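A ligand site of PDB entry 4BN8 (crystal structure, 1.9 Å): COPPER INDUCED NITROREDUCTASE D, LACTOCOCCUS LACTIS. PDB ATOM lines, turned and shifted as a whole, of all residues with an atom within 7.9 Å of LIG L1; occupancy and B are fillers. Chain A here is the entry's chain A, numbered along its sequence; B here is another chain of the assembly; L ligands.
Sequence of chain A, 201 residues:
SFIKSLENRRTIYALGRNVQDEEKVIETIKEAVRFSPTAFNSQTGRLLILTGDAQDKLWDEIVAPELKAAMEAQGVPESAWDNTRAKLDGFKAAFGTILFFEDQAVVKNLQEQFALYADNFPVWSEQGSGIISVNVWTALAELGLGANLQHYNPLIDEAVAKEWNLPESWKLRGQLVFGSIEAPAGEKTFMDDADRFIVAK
N2 of LG2 L2 is in hydrogen-bond range of O of Leu 149 of chain B (3.1 Å).
OG1 of Thr 11 of chain B sits at hydrogen-bond distance from O8 of LG2 L2, 2.7 Å away.
N of Phe 40 is in hydrogen-bond range of O1 of LIG L1, 2.9 Å away.
NE2 of Gln 150 of chain B sits at hydrogen-bond distance from O1 of LG2 L2 (3.0 Å).
O5 of LG2 L2 lies within hydrogen-bond range of N of Asn 41, at 3.5 Å.
The backbone NH (N) of Phe 40 is in hydrogen-bond range of an oxygen (O3) of LG2 L2, at 3.4 Å.
N of Thr 11 of chain B lies within hydrogen-bond range of O9 of LG2 L2, 2.7 Å away.
ND1 of His 151 of chain B lies within hydrogen-bond range of O2 of LG2 L2 (3.0 Å).
OH of Tyr 117 lies within hydrogen-bond range of O2 of LIG L1 (2.7 Å).
The backbone carbonyl oxygen (O) of Ala 39 is in hydrogen-bond range of the side-chain hydroxyl (OG) of Ser 42, 2.7 Å away.
The backbone carbonyl oxygen (O) of Tyr 117 lies close to the side-chain amide oxygen (OD1) of Asn 120 (3.5 Å).
Merely in contact with LIG L1: Ala 39 (3.8 Å).
Hydrophobic or aromatic side chains within 4 Å of LIG L1: Phe 40 and Tyr 117.
Of the 16 residues printed, 3 come within 4 Å of LIG L1.
An oxygen (O1) of LIG L1 is in hydrogen-bond range of an oxygen (O3) of LG2 L2 (3.1 Å).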
ATOM      1  N   THR A  38      -3.344 -29.778 -15.223  1.00  0.00           N
ATOM      2  CA  THR A  38      -3.322 -28.431 -15.757  1.00  0.00           C
ATOM      3  C   THR A  38      -2.990 -27.456 -14.630  1.00  0.00           C
ATOM      4  O   THR A  38      -3.337 -27.716 -13.480  1.00  0.00           O
ATOM      5  CB  THR A  38      -4.678 -28.023 -16.349  1.00  0.00           C
ATOM      6  OG1 THR A  38      -5.709 -28.209 -15.369  1.00  0.00           O
ATOM      7  CG2 THR A  38      -4.988 -28.851 -17.583  1.00  0.00           C
ATOM      8  N   ALA A  39      -2.312 -26.356 -14.951  1.00  0.00           N
ATOM      9  CA  ALA A  39      -1.962 -25.380 -13.937  1.00  0.00           C
ATOM     10  C   ALA A  39      -3.199 -24.983 -13.125  1.00  0.00           C
ATOM     11  O   ALA A  39      -4.257 -24.693 -13.682  1.00  0.00           O
ATOM     12  CB  ALA A  39      -1.328 -24.155 -14.570  1.00  0.00           C
ATOM     13  N   PHE A  40      -3.065 -25.015 -11.799  1.00  0.00           N
ATOM     14  CA  PHE A  40      -4.122 -24.555 -10.900  1.00  0.00           C
ATOM     15  C   PHE A  40      -5.374 -25.410 -11.066  1.00  0.00           C
ATOM     16  O   PHE A  40      -6.469 -25.012 -10.649  1.00  0.00           O
ATOM     17  CB  PHE A  40      -4.491 -23.095 -11.194  1.00  0.00           C
ATOM     18  CG  PHE A  40      -3.584 -22.084 -10.550  1.00  0.00           C
ATOM     19  CD1 PHE A  40      -2.297 -21.856 -11.031  1.00  0.00           C
ATOM     20  CD2 PHE A  40      -4.024 -21.327  -9.475  1.00  0.00           C
ATOM     21  CE1 PHE A  40      -1.473 -20.911 -10.437  1.00  0.00           C
ATOM     22  CE2 PHE A  40      -3.200 -20.382  -8.881  1.00  0.00           C
ATOM     23  CZ  PHE A  40      -1.924 -20.175  -9.367  1.00  0.00           C
ATOM     24  N   ASN A  41      -5.211 -26.591 -11.669  1.00  0.00           N
ATOM     25  CA  ASN A  41      -6.342 -27.454 -11.980  1.00  0.00           C
ATOM     26  C   ASN A  41      -7.388 -26.674 -12.772  1.00  0.00           C
ATOM     27  O   ASN A  41      -8.587 -26.862 -12.596  1.00  0.00           O
ATOM     28  CB  ASN A  41      -6.967 -27.990 -10.683  1.00  0.00           C
ATOM     29  CG  ASN A  41      -7.918 -29.147 -10.932  1.00  0.00           C
ATOM     30  OD1 ASN A  41      -7.724 -29.934 -11.859  1.00  0.00           O
ATOM     31  ND2 ASN A  41      -8.960 -29.253 -10.096  1.00  0.00           N
ATOM     32  N   SER A  42      -6.898 -25.803 -13.645  1.00  0.00           N
ATOM     33  CA  SER A  42      -7.742 -24.881 -14.399  1.00  0.00           C
ATOM     34  C   SER A  42      -8.553 -25.581 -15.508  1.00  0.00           C
ATOM     35  O   SER A  42      -9.592 -25.074 -15.932  1.00  0.00           O
ATOM     36  CB  SER A  42      -6.898 -23.753 -14.996  1.00  0.00           C
ATOM     37  OG  SER A  42      -5.833 -24.248 -15.782  1.00  0.00           O
ATOM     38  N   LEU A 116      -0.080 -11.572 -10.659  1.00  0.00           N
ATOM     39  CA  LEU A 116       1.352 -11.808 -10.560  1.00  0.00           C
ATOM     40  C   LEU A 116       1.806 -12.829 -11.610  1.00  0.00           C
ATOM     41  O   LEU A 116       2.906 -12.720 -12.154  1.00  0.00           O
ATOM     42  CB  LEU A 116       1.719 -12.313  -9.163  1.00  0.00           C
ATOM     43  CG  LEU A 116       3.012 -11.751  -8.571  1.00  0.00           C
ATOM     44  CD1 LEU A 116       2.790 -10.321  -8.075  1.00  0.00           C
ATOM     45  CD2 LEU A 116       3.518 -12.640  -7.451  1.00  0.00           C
ATOM     46  N   TYR A 117       0.953 -13.806 -11.878  1.00  0.00           N
ATOM     47  CA  TYR A 117       1.273 -14.876 -12.809  1.00  0.00           C
ATOM     48  C   TYR A 117       0.625 -14.665 -14.180  1.00  0.00           C
ATOM     49  O   TYR A 117       0.545 -15.588 -14.985  1.00  0.00           O
ATOM     50  CB  TYR A 117       0.804 -16.213 -12.221  1.00  0.00           C
ATOM     51  CG  TYR A 117       1.534 -16.614 -10.954  1.00  0.00           C
ATOM     52  CD1 TYR A 117       2.772 -17.232 -11.018  1.00  0.00           C
ATOM     53  CD2 TYR A 117       0.973 -16.383  -9.711  1.00  0.00           C
ATOM     54  CE1 TYR A 117       3.444 -17.605  -9.874  1.00  0.00           C
ATOM     55  CE2 TYR A 117       1.643 -16.764  -8.556  1.00  0.00           C
ATOM     56  CZ  TYR A 117       2.874 -17.366  -8.645  1.00  0.00           C
ATOM     57  OH  TYR A 117       3.546 -17.739  -7.501  1.00  0.00           O
ATOM     58  N   ASN A 120       2.153 -16.206 -17.165  1.00  0.00           N
ATOM     59  CA  ASN A 120       2.342 -17.645 -17.124  1.00  0.00           C
ATOM     60  C   ASN A 120       1.151 -18.458 -17.637  1.00  0.00           C
ATOM     61  O   ASN A 120       1.323 -19.523 -18.228  1.00  0.00           O
ATOM     62  CB  ASN A 120       2.673 -18.077 -15.695  1.00  0.00           C
ATOM     63  CG  ASN A 120       3.892 -17.373 -15.153  1.00  0.00           C
ATOM     64  OD1 ASN A 120       3.801 -16.567 -14.225  1.00  0.00           O
ATOM     65  ND2 ASN A 120       5.059 -17.672 -15.724  1.00  0.00           N
ATOM     66  N   PHE A 121      -0.061 -17.959 -17.408  1.00  0.00           N
ATOM     67  CA  PHE A 121      -1.246 -18.754 -17.719  1.00  0.00           C
ATOM     68  C   PHE A 121      -1.392 -19.101 -19.199  1.00  0.00           C
ATOM     69  O   PHE A 121      -1.759 -20.230 -19.535  1.00  0.00           O
ATOM     70  CB  PHE A 121      -2.505 -18.062 -17.189  1.00  0.00           C
ATOM     71  CG  PHE A 121      -2.570 -18.030 -15.694  1.00  0.00           C
ATOM     72  CD1 PHE A 121      -2.673 -19.208 -14.970  1.00  0.00           C
ATOM     73  CD2 PHE A 121      -2.506 -16.834 -15.009  1.00  0.00           C
ATOM     74  CE1 PHE A 121      -2.711 -19.195 -13.581  1.00  0.00           C
ATOM     75  CE2 PHE A 121      -2.554 -16.808 -13.614  1.00  0.00           C
ATOM     76  CZ  PHE A 121      -2.656 -17.991 -12.910  1.00  0.00           C
ATOM     77  N   TRP A 124       1.162 -21.838 -19.720  1.00  0.00           N
ATOM     78  CA  TRP A 124       0.719 -23.092 -19.121  1.00  0.00           C
ATOM     79  C   TRP A 124      -0.472 -23.673 -19.868  1.00  0.00           C
ATOM     80  O   TRP A 124      -0.649 -24.886 -19.914  1.00  0.00           O
ATOM     81  CB  TRP A 124       0.390 -22.880 -17.643  1.00  0.00           C
ATOM     82  CG  TRP A 124       1.583 -22.551 -16.822  1.00  0.00           C
ATOM     83  CD1 TRP A 124       2.884 -22.883 -17.089  1.00  0.00           C
ATOM     84  CD2 TRP A 124       1.604 -21.807 -15.593  1.00  0.00           C
ATOM     85  NE1 TRP A 124       3.717 -22.393 -16.112  1.00  0.00           N
ATOM     86  CE2 TRP A 124       2.956 -21.738 -15.173  1.00  0.00           C
ATOM     87  CE3 TRP A 124       0.619 -21.207 -14.809  1.00  0.00           C
ATOM     88  CZ2 TRP A 124       3.336 -21.080 -14.005  1.00  0.00           C
ATOM     89  CZ3 TRP A 124       0.998 -20.560 -13.648  1.00  0.00           C
ATOM     90  CH2 TRP A 124       2.343 -20.498 -13.258  1.00  0.00           C
ATOM     91  N   THR B  11       0.031 -34.734  -8.036  1.00  0.00           N
ATOM     92  CA  THR B  11       0.939 -33.814  -7.380  1.00  0.00           C
ATOM     93  C   THR B  11       1.155 -34.294  -5.946  1.00  0.00           C
ATOM     94  O   THR B  11       0.207 -34.391  -5.159  1.00  0.00           O
ATOM     95  CB  THR B  11       0.382 -32.383  -7.368  1.00  0.00           C
ATOM     96  OG1 THR B  11       0.445 -31.834  -8.690  1.00  0.00           O
ATOM     97  CG2 THR B  11       1.151 -31.495  -6.401  1.00  0.00           C
ATOM     98  N   TYR B  13       3.396 -33.263  -2.681  1.00  0.00           N
ATOM     99  CA  TYR B  13       4.284 -32.270  -2.075  1.00  0.00           C
ATOM    100  C   TYR B  13       5.206 -32.833  -1.004  1.00  0.00           C
ATOM    101  O   TYR B  13       6.335 -32.348  -0.845  1.00  0.00           O
ATOM    102  CB  TYR B  13       3.491 -31.084  -1.519  1.00  0.00           C
ATOM    103  CG  TYR B  13       2.910 -30.210  -2.608  1.00  0.00           C
ATOM    104  CD1 TYR B  13       3.748 -29.484  -3.455  1.00  0.00           C
ATOM    105  CD2 TYR B  13       1.544 -30.115  -2.791  1.00  0.00           C
ATOM    106  CE1 TYR B  13       3.214 -28.688  -4.460  1.00  0.00           C
ATOM    107  CE2 TYR B  13       1.008 -29.327  -3.784  1.00  0.00           C
ATOM    108  CZ  TYR B  13       1.844 -28.608  -4.619  1.00  0.00           C
ATOM    109  OH  TYR B  13       1.310 -27.822  -5.621  1.00  0.00           O
ATOM    110  N   LEU B 149       5.430 -30.166  -9.839  1.00  0.00           N
ATOM    111  CA  LEU B 149       5.992 -29.337 -10.893  1.00  0.00           C
ATOM    112  C   LEU B 149       5.999 -27.878 -10.474  1.00  0.00           C
ATOM    113  O   LEU B 149       4.950 -27.296 -10.174  1.00  0.00           O
ATOM    114  CB  LEU B 149       5.162 -29.496 -12.170  1.00  0.00           C
ATOM    115  CG  LEU B 149       5.612 -28.695 -13.389  1.00  0.00           C
ATOM    116  CD1 LEU B 149       7.010 -29.072 -13.794  1.00  0.00           C
ATOM    117  CD2 LEU B 149       4.648 -28.890 -14.531  1.00  0.00           C
ATOM    118  N   GLN B 150       7.191 -27.284 -10.474  1.00  0.00           N
ATOM    119  CA  GLN B 150       7.369 -25.907 -10.014  1.00  0.00           C
ATOM    120  C   GLN B 150       7.862 -25.017 -11.150  1.00  0.00           C
ATOM    121  O   GLN B 150       8.361 -25.507 -12.165  1.00  0.00           O
ATOM    122  CB  GLN B 150       8.390 -25.873  -8.871  1.00  0.00           C
ATOM    123  CG  GLN B 150       7.951 -26.656  -7.656  1.00  0.00           C
ATOM    124  CD  GLN B 150       6.583 -26.212  -7.174  1.00  0.00           C
ATOM    125  OE1 GLN B 150       6.293 -25.015  -7.109  1.00  0.00           O
ATOM    126  NE2 GLN B 150       5.736 -27.168  -6.847  1.00  0.00           N
ATOM    127  N   HIS B 151       7.733 -23.716 -10.968  1.00  0.00           N
ATOM    128  CA  HIS B 151       8.161 -22.756 -11.969  1.00  0.00           C
ATOM    129  C   HIS B 151       8.884 -21.565 -11.350  1.00  0.00           C
ATOM    130  O   HIS B 151       8.294 -20.520 -11.109  1.00  0.00           O
ATOM    131  CB  HIS B 151       6.958 -22.300 -12.802  1.00  0.00           C
ATOM    132  CG  HIS B 151       6.360 -23.396 -13.614  1.00  0.00           C
ATOM    133  ND1 HIS B 151       5.405 -24.263 -13.099  1.00  0.00           N
ATOM    134  CD2 HIS B 151       6.603 -23.813 -14.869  1.00  0.00           C
ATOM    135  CE1 HIS B 151       5.077 -25.137 -14.024  1.00  0.00           C
ATOM    136  NE2 HIS B 151       5.790 -24.893 -15.119  1.00  0.00           N
ATOM    137  N   TYR B 152      10.164 -21.750 -11.066  1.00  0.00           N
ATOM    138  CA  TYR B 152      10.992 -20.680 -10.514  1.00  0.00           C
ATOM    139  C   TYR B 152      11.833 -20.026 -11.611  1.00  0.00           C
ATOM    140  O   TYR B 152      12.666 -19.162 -11.347  1.00  0.00           O
ATOM    141  CB  TYR B 152      11.861 -21.210  -9.371  1.00  0.00           C
ATOM    142  CG  TYR B 152      11.049 -21.557  -8.153  1.00  0.00           C
ATOM    143  CD1 TYR B 152      10.511 -20.556  -7.350  1.00  0.00           C
ATOM    144  CD2 TYR B 152      10.802 -22.874  -7.805  1.00  0.00           C
ATOM    145  CE1 TYR B 152       9.761 -20.863  -6.231  1.00  0.00           C
ATOM    146  CE2 TYR B 152      10.040 -23.189  -6.684  1.00  0.00           C
ATOM    147  CZ  TYR B 152       9.526 -22.175  -5.904  1.00  0.00           C
ATOM    148  OH  TYR B 152       8.776 -22.472  -4.788  1.00  0.00           O
HETATM  149  C1  LIG L   1       1.492 -22.004  -7.909  1.00  0.00           C
HETATM  150  C2  LIG L   1       1.493 -21.867  -9.296  1.00  0.00           C
HETATM  151  C3  LIG L   1       0.750 -22.741 -10.068  1.00  0.00           C
HETATM  152  C4  LIG L   1       0.016 -23.753  -9.453  1.00  0.00           C
HETATM  153  C5  LIG L   1       0.016 -23.882  -8.078  1.00  0.00           C
HETATM  154  C6  LIG L   1       0.757 -23.015  -7.294  1.00  0.00           C
HETATM  155  O1  LIG L   1      -0.729 -24.619 -10.196  1.00  0.00           O
HETATM  156  N1  LIG L   1       2.256 -21.095  -7.113  1.00  0.00           N
HETATM  157  O2  LIG L   1       3.089 -20.363  -7.642  1.00  0.00           O
HETATM  158  O3  LIG L   1       2.067 -21.061  -5.831  1.00  0.00           O
HETATM  159  N1  LG2 L   2       1.873 -26.962  -9.213  1.00  0.00           N
HETATM  160  C1  LG2 L   2       2.714 -26.107  -8.307  1.00  0.00           C
HETATM  161  O1  LG2 L   2       2.811 -26.363  -7.153  1.00  0.00           O
HETATM  162  N2  LG2 L   2       3.414 -24.972  -8.852  1.00  0.00           N
HETATM  163  C2  LG2 L   2       3.326 -24.642 -10.168  1.00  0.00           C
HETATM  164  O2  LG2 L   2       3.926 -23.727 -10.602  1.00  0.00           O
HETATM  165  C3  LG2 L   2       2.505 -25.475 -11.059  1.00  0.00           C
HETATM  166  N3  LG2 L   2       2.397 -25.195 -12.292  1.00  0.00           N
HETATM  167  C4  LG2 L   2       1.815 -26.222 -13.233  1.00  0.00           C
HETATM  168  C5  LG2 L   2       1.970 -26.038 -14.737  1.00  0.00           C
HETATM  169  C6  LG2 L   2       1.471 -26.941 -15.561  1.00  0.00           C
HETATM  170  C7  LG2 L   2       1.607 -26.757 -17.076  1.00  0.00           C
HETATM  171  C8  LG2 L   2       0.743 -28.166 -15.015  1.00  0.00           C
HETATM  172  C9  LG2 L   2       0.191 -29.212 -15.982  1.00  0.00           C
HETATM  173  C10 LG2 L   2       0.595 -28.328 -13.713  1.00  0.00           C
HETATM  174  C11 LG2 L   2       1.166 -27.296 -12.752  1.00  0.00           C
HETATM  175  N4  LG2 L   2       1.008 -27.470 -11.334  1.00  0.00           N
HETATM  176  C12 LG2 L   2       1.779 -26.664 -10.491  1.00  0.00           C
HETATM  177  C13 LG2 L   2       0.326 -28.627 -10.783  1.00  0.00           C
HETATM  178  C14 LG2 L   2      -1.190 -28.519 -10.978  1.00  0.00           C
HETATM  179  O3  LG2 L   2      -1.741 -27.585 -10.077  1.00  0.00           O
HETATM  180  C15 LG2 L   2      -1.808 -29.887 -10.710  1.00  0.00           C
HETATM  181  O4  LG2 L   2      -1.321 -30.795 -11.663  1.00  0.00           O
HETATM  182  C16 LG2 L   2      -3.341 -29.785 -10.812  1.00  0.00           C
HETATM  183  O5  LG2 L   2      -3.830 -29.087  -9.704  1.00  0.00           O
HETATM  184  C17 LG2 L   2      -3.960 -31.178 -10.817  1.00  0.00           C
HETATM  185  O6  LG2 L   2      -3.558 -31.851  -9.665  1.00  0.00           O
HETATM  186  P1  LG2 L   2      -2.702 -33.245  -9.856  1.00  0.00           P
HETATM  187  O7  LG2 L   2      -3.426 -34.144 -10.765  1.00  0.00           O
HETATM  188  O8  LG2 L   2      -1.239 -32.890 -10.502  1.00  0.00           O
HETATM  189  O9  LG2 L   2      -2.550 -33.958  -8.387  1.00  0.00           O
